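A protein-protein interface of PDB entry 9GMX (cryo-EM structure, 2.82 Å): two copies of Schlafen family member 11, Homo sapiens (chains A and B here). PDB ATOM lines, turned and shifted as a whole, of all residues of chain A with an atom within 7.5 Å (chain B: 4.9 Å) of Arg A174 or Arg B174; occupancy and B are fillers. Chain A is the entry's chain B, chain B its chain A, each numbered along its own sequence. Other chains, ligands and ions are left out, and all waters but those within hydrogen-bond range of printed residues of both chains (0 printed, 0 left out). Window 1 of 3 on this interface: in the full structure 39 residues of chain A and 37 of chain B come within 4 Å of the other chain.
The guanidinium group (NH1) of Arg B174 lies close to the guanidinium group (NH1) of Arg A174.
OE2 of Glu A175 lies close to O of Gln B114, at 3.2 Å.
The side-chain amide oxygen of Gln B114 lies close to the side-chain carboxylate of Asp B172, at 2.6 Å.
The backbone NH (N) of Ser B173 lies within hydrogen-bond range of the side-chain amide oxygen (OE1) of Gln B114 (3.2 Å).
The backbone NH (N) of Arg A174 sits at hydrogen-bond distance from the side-chain amide oxygen (OE1) of Gln A114 (2.8 Å).
The side-chain carboxylate (OE1) of Glu A175 is in salt-bridge range of the guanidinium group (NH1) of Arg A162, at 3.4 Å.
The side-chain carboxylate of Asp A172 sits at hydrogen-bond distance from the backbone NH of Glu A175 (3.1 Å).
The backbone carbonyl oxygen (O) of Arg A174 sits at hydrogen-bond distance from the side-chain sulfur (SG) of Cys A178.
Among the printed residues, merely in contact across the chains: Ser A115 with Glu B175 (3.6 Å) and Val A149 with Val B149 (3.6 Å).
Of chain B, only Arg B174 (2.8 Å) comes within 4 Å of Arg A174.
Of chain A, only Arg A174 comes within 4 Å of Arg B174.
Printed residues of chain A within 4 Å of Val B149: Val A149.
Of the printed residues of chain B, Glu A175 touches Gln B114 (3.2 Å).
The nearest printed residue of chain B that does not touch Val A149 is Arg B174 (7.6 Å).
Hydrophobic or aromatic side chains of chain A that line the printed part of chain B: Val A149.
Among the printed residues, no Asp or Glu carboxylate lies within 4 Å of a Lys or Arg side-chain nitrogen of the other chain.
Val A149 touches its own counterpart, Val B149.
Arg A174 touches its own counterpart, Arg B174.
Glu A175 touches Gln B114, but with the chains exchanged Gln A114 does not touch Glu B175 (5.1 Å).
Of the 4 pairs that touch across the chains among the printed residues, 2 have their exchanged pair printed and touching as well.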
ATOM      1  N   ILE A 113      10.377 -17.216 -13.508  1.00  0.00           N
ATOM      2  CA  ILE A 113       9.078 -16.771 -13.006  1.00  0.00           C
ATOM      3  C   ILE A 113       8.156 -17.920 -12.615  1.00  0.00           C
ATOM      4  O   ILE A 113       7.013 -17.670 -12.216  1.00  0.00           O
ATOM      5  CB  ILE A 113       8.355 -15.875 -14.028  1.00  0.00           C
ATOM      6  CG1 ILE A 113       8.186 -16.595 -15.359  1.00  0.00           C
ATOM      7  CG2 ILE A 113       9.111 -14.589 -14.195  1.00  0.00           C
ATOM      8  CD1 ILE A 113       7.116 -16.007 -16.230  1.00  0.00           C
ATOM      9  N   GLN A 114       8.614 -19.165 -12.711  1.00  0.00           N
ATOM     10  CA  GLN A 114       7.832 -20.338 -12.328  1.00  0.00           C
ATOM     11  C   GLN A 114       6.474 -20.365 -13.020  1.00  0.00           C
ATOM     12  O   GLN A 114       5.463 -20.744 -12.433  1.00  0.00           O
ATOM     13  CB  GLN A 114       7.660 -20.398 -10.821  1.00  0.00           C
ATOM     14  CG  GLN A 114       8.944 -20.512 -10.070  1.00  0.00           C
ATOM     15  CD  GLN A 114       8.745 -21.108  -8.710  1.00  0.00           C
ATOM     16  OE1 GLN A 114       8.968 -20.452  -7.704  1.00  0.00           O
ATOM     17  NE2 GLN A 114       8.307 -22.356  -8.668  1.00  0.00           N
ATOM     18  N   SER A 115       6.452 -19.981 -14.288  1.00  0.00           N
ATOM     19  CA  SER A 115       5.210 -19.907 -15.033  1.00  0.00           C
ATOM     20  C   SER A 115       5.535 -19.866 -16.509  1.00  0.00           C
ATOM     21  O   SER A 115       6.599 -19.394 -16.908  1.00  0.00           O
ATOM     22  CB  SER A 115       4.398 -18.670 -14.642  1.00  0.00           C
ATOM     23  OG  SER A 115       3.185 -18.589 -15.359  1.00  0.00           O
ATOM     24  N   TRP A 138       9.098  -8.395  -9.832  1.00  0.00           N
ATOM     25  CA  TRP A 138       8.461  -9.595  -9.315  1.00  0.00           C
ATOM     26  C   TRP A 138       7.432  -9.250  -8.248  1.00  0.00           C
ATOM     27  O   TRP A 138       6.236  -9.505  -8.418  1.00  0.00           O
ATOM     28  CB  TRP A 138       9.522 -10.537  -8.761  1.00  0.00           C
ATOM     29  CG  TRP A 138       8.974 -11.764  -8.147  1.00  0.00           C
ATOM     30  CD1 TRP A 138       9.101 -12.158  -6.858  1.00  0.00           C
ATOM     31  CD2 TRP A 138       8.195 -12.765  -8.800  1.00  0.00           C
ATOM     32  NE1 TRP A 138       8.458 -13.345  -6.663  1.00  0.00           N
ATOM     33  CE2 TRP A 138       7.890 -13.739  -7.843  1.00  0.00           C
ATOM     34  CE3 TRP A 138       7.725 -12.932 -10.106  1.00  0.00           C
ATOM     35  CZ2 TRP A 138       7.143 -14.868  -8.147  1.00  0.00           C
ATOM     36  CZ3 TRP A 138       6.985 -14.045 -10.399  1.00  0.00           C
ATOM     37  CH2 TRP A 138       6.701 -14.998  -9.428  1.00  0.00           C
ATOM     38  N   VAL A 149       1.800 -15.579   0.248  1.00  0.00           N
ATOM     39  CA  VAL A 149       1.403 -16.442  -0.855  1.00  0.00           C
ATOM     40  C   VAL A 149       2.556 -16.716  -1.811  1.00  0.00           C
ATOM     41  O   VAL A 149       2.777 -17.866  -2.204  1.00  0.00           O
ATOM     42  CB  VAL A 149       0.200 -15.836  -1.612  1.00  0.00           C
ATOM     43  CG1 VAL A 149       0.189 -16.258  -3.073  1.00  0.00           C
ATOM     44  CG2 VAL A 149      -1.092 -16.248  -0.946  1.00  0.00           C
ATOM     45  N   LYS A 150       3.297 -15.685  -2.205  1.00  0.00           N
ATOM     46  CA  LYS A 150       4.374 -15.814  -3.170  1.00  0.00           C
ATOM     47  C   LYS A 150       5.663 -15.264  -2.583  1.00  0.00           C
ATOM     48  O   LYS A 150       5.631 -14.383  -1.722  1.00  0.00           O
ATOM     49  CB  LYS A 150       4.044 -15.078  -4.476  1.00  0.00           C
ATOM     50  CG  LYS A 150       4.180 -13.594  -4.361  1.00  0.00           C
ATOM     51  CD  LYS A 150       3.726 -12.858  -5.595  1.00  0.00           C
ATOM     52  CE  LYS A 150       4.800 -12.842  -6.640  1.00  0.00           C
ATOM     53  NZ  LYS A 150       4.482 -11.908  -7.746  1.00  0.00           N
ATOM     54  N   PRO A 151       6.811 -15.771  -3.024  1.00  0.00           N
ATOM     55  CA  PRO A 151       8.082 -15.321  -2.452  1.00  0.00           C
ATOM     56  C   PRO A 151       8.481 -13.903  -2.820  1.00  0.00           C
ATOM     57  O   PRO A 151       8.026 -13.336  -3.816  1.00  0.00           O
ATOM     58  CB  PRO A 151       9.092 -16.336  -2.994  1.00  0.00           C
ATOM     59  CG  PRO A 151       8.471 -16.890  -4.191  1.00  0.00           C
ATOM     60  CD  PRO A 151       7.001 -16.862  -3.994  1.00  0.00           C
ATOM     61  N   LEU A 153      11.609 -12.877  -3.615  1.00  0.00           N
ATOM     62  CA  LEU A 153      12.621 -12.863  -4.651  1.00  0.00           C
ATOM     63  C   LEU A 153      12.382 -13.914  -5.719  1.00  0.00           C
ATOM     64  O   LEU A 153      11.812 -14.973  -5.457  1.00  0.00           O
ATOM     65  CB  LEU A 153      13.965 -13.153  -3.998  1.00  0.00           C
ATOM     66  CG  LEU A 153      14.459 -12.174  -2.955  1.00  0.00           C
ATOM     67  CD1 LEU A 153      15.682 -12.742  -2.306  1.00  0.00           C
ATOM     68  CD2 LEU A 153      14.743 -10.842  -3.596  1.00  0.00           C
ATOM     69  N   ARG A 162      16.057 -31.089  -1.334  1.00  0.00           N
ATOM     70  CA  ARG A 162      15.276 -32.060  -0.642  1.00  0.00           C
ATOM     71  C   ARG A 162      15.350 -33.481  -1.073  1.00  0.00           C
ATOM     72  O   ARG A 162      15.399 -33.718  -2.221  1.00  0.00           O
ATOM     73  CB  ARG A 162      13.832 -31.678  -0.860  1.00  0.00           C
ATOM     74  CG  ARG A 162      12.741 -32.462  -0.209  1.00  0.00           C
ATOM     75  CD  ARG A 162      11.446 -31.841  -0.679  1.00  0.00           C
ATOM     76  NE  ARG A 162      11.211 -30.490  -0.198  1.00  0.00           N
ATOM     77  CZ  ARG A 162      10.182 -29.738  -0.548  1.00  0.00           C
ATOM     78  NH1 ARG A 162       9.270 -30.206  -1.371  1.00  0.00           N
ATOM     79  NH2 ARG A 162      10.072 -28.514  -0.077  1.00  0.00           N
ATOM     80  N   MET A 171      14.762 -27.075  -4.473  1.00  0.00           N
ATOM     81  CA  MET A 171      13.516 -26.375  -4.217  1.00  0.00           C
ATOM     82  C   MET A 171      13.446 -25.118  -5.067  1.00  0.00           C
ATOM     83  O   MET A 171      14.308 -24.244  -4.958  1.00  0.00           O
ATOM     84  CB  MET A 171      13.421 -26.012  -2.743  1.00  0.00           C
ATOM     85  CG  MET A 171      13.109 -27.160  -1.821  1.00  0.00           C
ATOM     86  SD  MET A 171      12.929 -26.574  -0.143  1.00  0.00           S
ATOM     87  CE  MET A 171      13.975 -27.719   0.720  1.00  0.00           C
ATOM     88  N   ASP A 172      12.427 -25.017  -5.911  1.00  0.00           N
ATOM     89  CA  ASP A 172      12.197 -23.775  -6.623  1.00  0.00           C
ATOM     90  C   ASP A 172      11.803 -22.696  -5.623  1.00  0.00           C
ATOM     91  O   ASP A 172      11.724 -22.938  -4.430  1.00  0.00           O
ATOM     92  CB  ASP A 172      11.140 -23.971  -7.705  1.00  0.00           C
ATOM     93  CG  ASP A 172       9.865 -24.577  -7.179  1.00  0.00           C
ATOM     94  OD1 ASP A 172       9.010 -23.835  -6.663  1.00  0.00           O
ATOM     95  OD2 ASP A 172       9.722 -25.809  -7.272  1.00  0.00           O
ATOM     96  N   SER A 173      11.597 -21.475  -6.112  1.00  0.00           N
ATOM     97  CA  SER A 173      11.358 -20.368  -5.193  1.00  0.00           C
ATOM     98  C   SER A 173      10.118 -20.603  -4.347  1.00  0.00           C
ATOM     99  O   SER A 173      10.132 -20.352  -3.144  1.00  0.00           O
ATOM    100  CB  SER A 173      11.234 -19.056  -5.957  1.00  0.00           C
ATOM    101  OG  SER A 173      12.448 -18.722  -6.588  1.00  0.00           O
ATOM    102  N   ARG A 174       9.039 -21.088  -4.954  1.00  0.00           N
ATOM    103  CA  ARG A 174       7.807 -21.340  -4.212  1.00  0.00           C
ATOM    104  C   ARG A 174       7.989 -22.450  -3.181  1.00  0.00           C
ATOM    105  O   ARG A 174       7.549 -22.325  -2.032  1.00  0.00           O
ATOM    106  CB  ARG A 174       6.704 -21.700  -5.197  1.00  0.00           C
ATOM    107  CG  ARG A 174       5.417 -20.968  -4.998  1.00  0.00           C
ATOM    108  CD  ARG A 174       4.291 -21.669  -5.712  1.00  0.00           C
ATOM    109  NE  ARG A 174       4.145 -21.234  -7.096  1.00  0.00           N
ATOM    110  CZ  ARG A 174       4.560 -21.912  -8.158  1.00  0.00           C
ATOM    111  NH1 ARG A 174       5.260 -23.028  -8.043  1.00  0.00           N
ATOM    112  NH2 ARG A 174       4.265 -21.457  -9.372  1.00  0.00           N
ATOM    113  N   GLU A 175       8.635 -23.545  -3.578  1.00  0.00           N
ATOM    114  CA  GLU A 175       8.904 -24.641  -2.657  1.00  0.00           C
ATOM    115  C   GLU A 175       9.756 -24.179  -1.490  1.00  0.00           C
ATOM    116  O   GLU A 175       9.490 -24.525  -0.337  1.00  0.00           O
ATOM    117  CB  GLU A 175       9.623 -25.764  -3.392  1.00  0.00           C
ATOM    118  CG  GLU A 175       8.841 -26.449  -4.479  1.00  0.00           C
ATOM    119  CD  GLU A 175       7.556 -27.044  -3.948  1.00  0.00           C
ATOM    120  OE1 GLU A 175       7.565 -27.604  -2.828  1.00  0.00           O
ATOM    121  OE2 GLU A 175       6.544 -26.989  -4.675  1.00  0.00           O
ATOM    122  N   ALA A 176      10.813 -23.417  -1.777  1.00  0.00           N
ATOM    123  CA  ALA A 176      11.708 -22.948  -0.727  1.00  0.00           C
ATOM    124  C   ALA A 176      11.018 -21.930   0.163  1.00  0.00           C
ATOM    125  O   ALA A 176      11.273 -21.872   1.367  1.00  0.00           O
ATOM    126  CB  ALA A 176      12.965 -22.351  -1.347  1.00  0.00           C
ATOM    127  N   PHE A 177      10.139 -21.120  -0.414  1.00  0.00           N
ATOM    128  CA  PHE A 177       9.352 -20.189   0.374  1.00  0.00           C
ATOM    129  C   PHE A 177       8.511 -20.936   1.390  1.00  0.00           C
ATOM    130  O   PHE A 177       8.533 -20.624   2.582  1.00  0.00           O
ATOM    131  CB  PHE A 177       8.474 -19.365  -0.562  1.00  0.00           C
ATOM    132  CG  PHE A 177       7.556 -18.429   0.135  1.00  0.00           C
ATOM    133  CD1 PHE A 177       8.055 -17.431   0.941  1.00  0.00           C
ATOM    134  CD2 PHE A 177       6.195 -18.538  -0.019  1.00  0.00           C
ATOM    135  CE1 PHE A 177       7.216 -16.568   1.581  1.00  0.00           C
ATOM    136  CE2 PHE A 177       5.354 -17.677   0.621  1.00  0.00           C
ATOM    137  CZ  PHE A 177       5.866 -16.689   1.423  1.00  0.00           C
ATOM    138  N   CYS A 178       7.777 -21.949   0.934  1.00  0.00           N
ATOM    139  CA  CYS A 178       6.963 -22.741   1.850  1.00  0.00           C
ATOM    140  C   CYS A 178       7.826 -23.470   2.870  1.00  0.00           C
ATOM    141  O   CYS A 178       7.466 -23.565   4.047  1.00  0.00           O
ATOM    142  CB  CYS A 178       6.115 -23.725   1.056  1.00  0.00           C
ATOM    143  SG  CYS A 178       4.873 -22.929   0.035  1.00  0.00           S
ATOM    144  N   PHE A 179       8.972 -23.986   2.438  1.00  0.00           N
ATOM    145  CA  PHE A 179       9.869 -24.703   3.333  1.00  0.00           C
ATOM    146  C   PHE A 179      10.359 -23.811   4.467  1.00  0.00           C
ATOM    147  O   PHE A 179      10.331 -24.198   5.639  1.00  0.00           O
ATOM    148  CB  PHE A 179      11.039 -25.234   2.515  1.00  0.00           C
ATOM    149  CG  PHE A 179      12.125 -25.849   3.324  1.00  0.00           C
ATOM    150  CD1 PHE A 179      11.969 -27.101   3.877  1.00  0.00           C
ATOM    151  CD2 PHE A 179      13.313 -25.184   3.516  1.00  0.00           C
ATOM    152  CE1 PHE A 179      12.973 -27.670   4.608  1.00  0.00           C
ATOM    153  CE2 PHE A 179      14.318 -25.751   4.249  1.00  0.00           C
ATOM    154  CZ  PHE A 179      14.149 -26.994   4.797  1.00  0.00           C
ATOM    155  N   LEU A 180      10.819 -22.608   4.135  1.00  0.00           N
ATOM    156  CA  LEU A 180      11.318 -21.702   5.160  1.00  0.00           C
ATOM    157  C   LEU A 180      10.185 -21.165   6.018  1.00  0.00           C
ATOM    158  O   LEU A 180      10.349 -20.978   7.226  1.00  0.00           O
ATOM    159  CB  LEU A 180      12.086 -20.560   4.505  1.00  0.00           C
ATOM    160  CG  LEU A 180      13.320 -20.951   3.703  1.00  0.00           C
ATOM    161  CD1 LEU A 180      13.837 -19.752   2.961  1.00  0.00           C
ATOM    162  CD2 LEU A 180      14.378 -21.507   4.612  1.00  0.00           C
ATOM    163  N   MET A 379      13.361 -13.760   1.849  1.00  0.00           N
ATOM    164  CA  MET A 379      12.412 -14.805   1.495  1.00  0.00           C
ATOM    165  C   MET A 379      11.458 -15.146   2.627  1.00  0.00           C
ATOM    166  O   MET A 379      10.401 -15.724   2.365  1.00  0.00           O
ATOM    167  CB  MET A 379      13.156 -16.063   1.054  1.00  0.00           C
ATOM    168  CG  MET A 379      13.682 -15.982  -0.362  1.00  0.00           C
ATOM    169  SD  MET A 379      12.376 -15.935  -1.586  1.00  0.00           S
ATOM    170  CE  MET A 379      12.042 -17.669  -1.772  1.00  0.00           C
ATOM    171  N   ILE B 113       1.556 -33.586  -7.676  1.00  0.00           N
ATOM    172  CA  ILE B 113       1.421 -32.648  -6.565  1.00  0.00           C
ATOM    173  C   ILE B 113       2.170 -31.341  -6.791  1.00  0.00           C
ATOM    174  O   ILE B 113       2.167 -30.481  -5.903  1.00  0.00           O
ATOM    175  CB  ILE B 113       1.879 -33.265  -5.227  1.00  0.00           C
ATOM    176  CG1 ILE B 113       3.313 -33.775  -5.308  1.00  0.00           C
ATOM    177  CG2 ILE B 113       0.936 -34.369  -4.819  1.00  0.00           C
ATOM    178  CD1 ILE B 113       3.955 -33.971  -3.976  1.00  0.00           C
ATOM    179  N   GLN B 114       2.798 -31.158  -7.953  1.00  0.00           N
ATOM    180  CA  GLN B 114       3.563 -29.952  -8.276  1.00  0.00           C
ATOM    181  C   GLN B 114       4.604 -29.639  -7.210  1.00  0.00           C
ATOM    182  O   GLN B 114       4.816 -28.484  -6.847  1.00  0.00           O
ATOM    183  CB  GLN B 114       2.651 -28.751  -8.486  1.00  0.00           C
ATOM    184  CG  GLN B 114       1.569 -28.945  -9.493  1.00  0.00           C
ATOM    185  CD  GLN B 114       0.504 -27.892  -9.365  1.00  0.00           C
ATOM    186  OE1 GLN B 114       0.391 -27.010 -10.208  1.00  0.00           O
ATOM    187  NE2 GLN B 114      -0.287 -27.972  -8.301  1.00  0.00           N
ATOM    188  N   VAL B 149      -5.964 -19.851  -2.963  1.00  0.00           N
ATOM    189  CA  VAL B 149      -4.575 -19.810  -3.390  1.00  0.00           C
ATOM    190  C   VAL B 149      -4.168 -21.084  -4.121  1.00  0.00           C
ATOM    191  O   VAL B 149      -3.402 -21.026  -5.084  1.00  0.00           O
ATOM    192  CB  VAL B 149      -3.645 -19.541  -2.187  1.00  0.00           C
ATOM    193  CG1 VAL B 149      -4.010 -18.221  -1.539  1.00  0.00           C
ATOM    194  CG2 VAL B 149      -3.719 -20.667  -1.174  1.00  0.00           C
ATOM    195  N   PRO B 151      -5.368 -24.911  -6.001  1.00  0.00           N
ATOM    196  CA  PRO B 151      -6.524 -25.530  -6.651  1.00  0.00           C
ATOM    197  C   PRO B 151      -7.118 -26.663  -5.834  1.00  0.00           C
ATOM    198  O   PRO B 151      -6.454 -27.286  -5.003  1.00  0.00           O
ATOM    199  CB  PRO B 151      -5.949 -26.039  -7.975  1.00  0.00           C
ATOM    200  CG  PRO B 151      -4.504 -26.158  -7.746  1.00  0.00           C
ATOM    201  CD  PRO B 151      -4.130 -25.119  -6.766  1.00  0.00           C
ATOM    202  N   ASP B 172      -0.018 -26.266 -15.575  1.00  0.00           N
ATOM    203  CA  ASP B 172      -0.203 -27.183 -14.466  1.00  0.00           C
ATOM    204  C   ASP B 172      -1.415 -26.756 -13.647  1.00  0.00           C
ATOM    205  O   ASP B 172      -2.136 -25.836 -14.005  1.00  0.00           O
ATOM    206  CB  ASP B 172       1.056 -27.245 -13.606  1.00  0.00           C
ATOM    207  CG  ASP B 172       1.535 -25.882 -13.173  1.00  0.00           C
ATOM    208  OD1 ASP B 172       1.606 -24.990 -14.039  1.00  0.00           O
ATOM    209  OD2 ASP B 172       1.850 -25.701 -11.978  1.00  0.00           O
ATOM    210  N   SER B 173      -1.668 -27.468 -12.550  1.00  0.00           N
ATOM    211  CA  SER B 173      -2.875 -27.192 -11.775  1.00  0.00           C
ATOM    212  C   SER B 173      -2.896 -25.758 -11.276  1.00  0.00           C
ATOM    213  O   SER B 173      -3.911 -25.069 -11.387  1.00  0.00           O
ATOM    214  CB  SER B 173      -2.984 -28.158 -10.599  1.00  0.00           C
ATOM    215  OG  SER B 173      -3.090 -29.499 -11.030  1.00  0.00           O
ATOM    216  N   ARG B 174      -1.780 -25.288 -10.727  1.00  0.00           N
ATOM    217  CA  ARG B 174      -1.716 -23.947 -10.163  1.00  0.00           C
ATOM    218  C   ARG B 174      -1.842 -22.882 -11.250  1.00  0.00           C
ATOM    219  O   ARG B 174      -2.560 -21.887 -11.083  1.00  0.00           O
ATOM    220  CB  ARG B 174      -0.402 -23.814  -9.409  1.00  0.00           C
ATOM    221  CG  ARG B 174      -0.318 -22.698  -8.432  1.00  0.00           C
ATOM    222  CD  ARG B 174       1.061 -22.664  -7.823  1.00  0.00           C
ATOM    223  NE  ARG B 174       1.283 -23.769  -6.899  1.00  0.00           N
ATOM    224  CZ  ARG B 174       2.208 -24.713  -7.035  1.00  0.00           C
ATOM    225  NH1 ARG B 174       3.041 -24.731  -8.062  1.00  0.00           N
ATOM    226  NH2 ARG B 174       2.299 -25.670  -6.115  1.00  0.00           N
ATOM    227  N   GLU B 175      -1.160 -23.084 -12.375  1.00  0.00           N
ATOM    228  CA  GLU B 175      -1.263 -22.163 -13.501  1.00  0.00           C
ATOM    229  C   GLU B 175      -2.682 -22.100 -14.038  1.00  0.00           C
ATOM    230  O   GLU B 175      -3.190 -21.021 -14.341  1.00  0.00           O
ATOM    231  CB  GLU B 175      -0.319 -22.602 -14.611  1.00  0.00           C
ATOM    232  CG  GLU B 175       1.035 -21.973 -14.597  1.00  0.00           C
ATOM    233  CD  GLU B 175       1.612 -21.880 -15.981  1.00  0.00           C
ATOM    234  OE1 GLU B 175       1.081 -21.108 -16.806  1.00  0.00           O
ATOM    235  OE2 GLU B 175       2.580 -22.613 -16.258  1.00  0.00           O
ATOM    236  N   ALA B 176      -3.326 -23.256 -14.199  1.00  0.00           N
ATOM    237  CA  ALA B 176      -4.689 -23.292 -14.716  1.00  0.00           C
ATOM    238  C   ALA B 176      -5.662 -22.679 -13.728  1.00  0.00           C
ATOM    239  O   ALA B 176      -6.639 -22.042 -14.122  1.00  0.00           O
ATOM    240  CB  ALA B 176      -5.088 -24.729 -15.035  1.00  0.00           C
ATOM    241  N   PHE B 177      -5.411 -22.862 -12.437  1.00  0.00           N
ATOM    242  CA  PHE B 177      -6.224 -22.225 -11.414  1.00  0.00           C
ATOM    243  C   PHE B 177      -6.171 -20.711 -11.551  1.00  0.00           C
ATOM    244  O   PHE B 177      -7.209 -20.042 -11.613  1.00  0.00           O
ATOM    245  CB  PHE B 177      -5.717 -22.678 -10.047  1.00  0.00           C
ATOM    246  CG  PHE B 177      -6.445 -22.091  -8.893  1.00  0.00           C
ATOM    247  CD1 PHE B 177      -7.734 -22.480  -8.603  1.00  0.00           C
ATOM    248  CD2 PHE B 177      -5.829 -21.172  -8.071  1.00  0.00           C
ATOM    249  CE1 PHE B 177      -8.396 -21.949  -7.526  1.00  0.00           C
ATOM    250  CE2 PHE B 177      -6.490 -20.639  -6.999  1.00  0.00           C
ATOM    251  CZ  PHE B 177      -7.773 -21.030  -6.726  1.00  0.00           C
ATOM    252  N   CYS B 178      -4.961 -20.155 -11.627  1.00  0.00           N
ATOM    253  CA  CYS B 178      -4.818 -18.711 -11.772  1.00  0.00           C
ATOM    254  C   CYS B 178      -5.397 -18.220 -13.091  1.00  0.00           C
ATOM    255  O   CYS B 178      -6.025 -17.157 -13.144  1.00  0.00           O
ATOM    256  CB  CYS B 178      -3.349 -18.321 -11.653  1.00  0.00           C
ATOM    257  SG  CYS B 178      -2.649 -18.656 -10.038  1.00  0.00           S
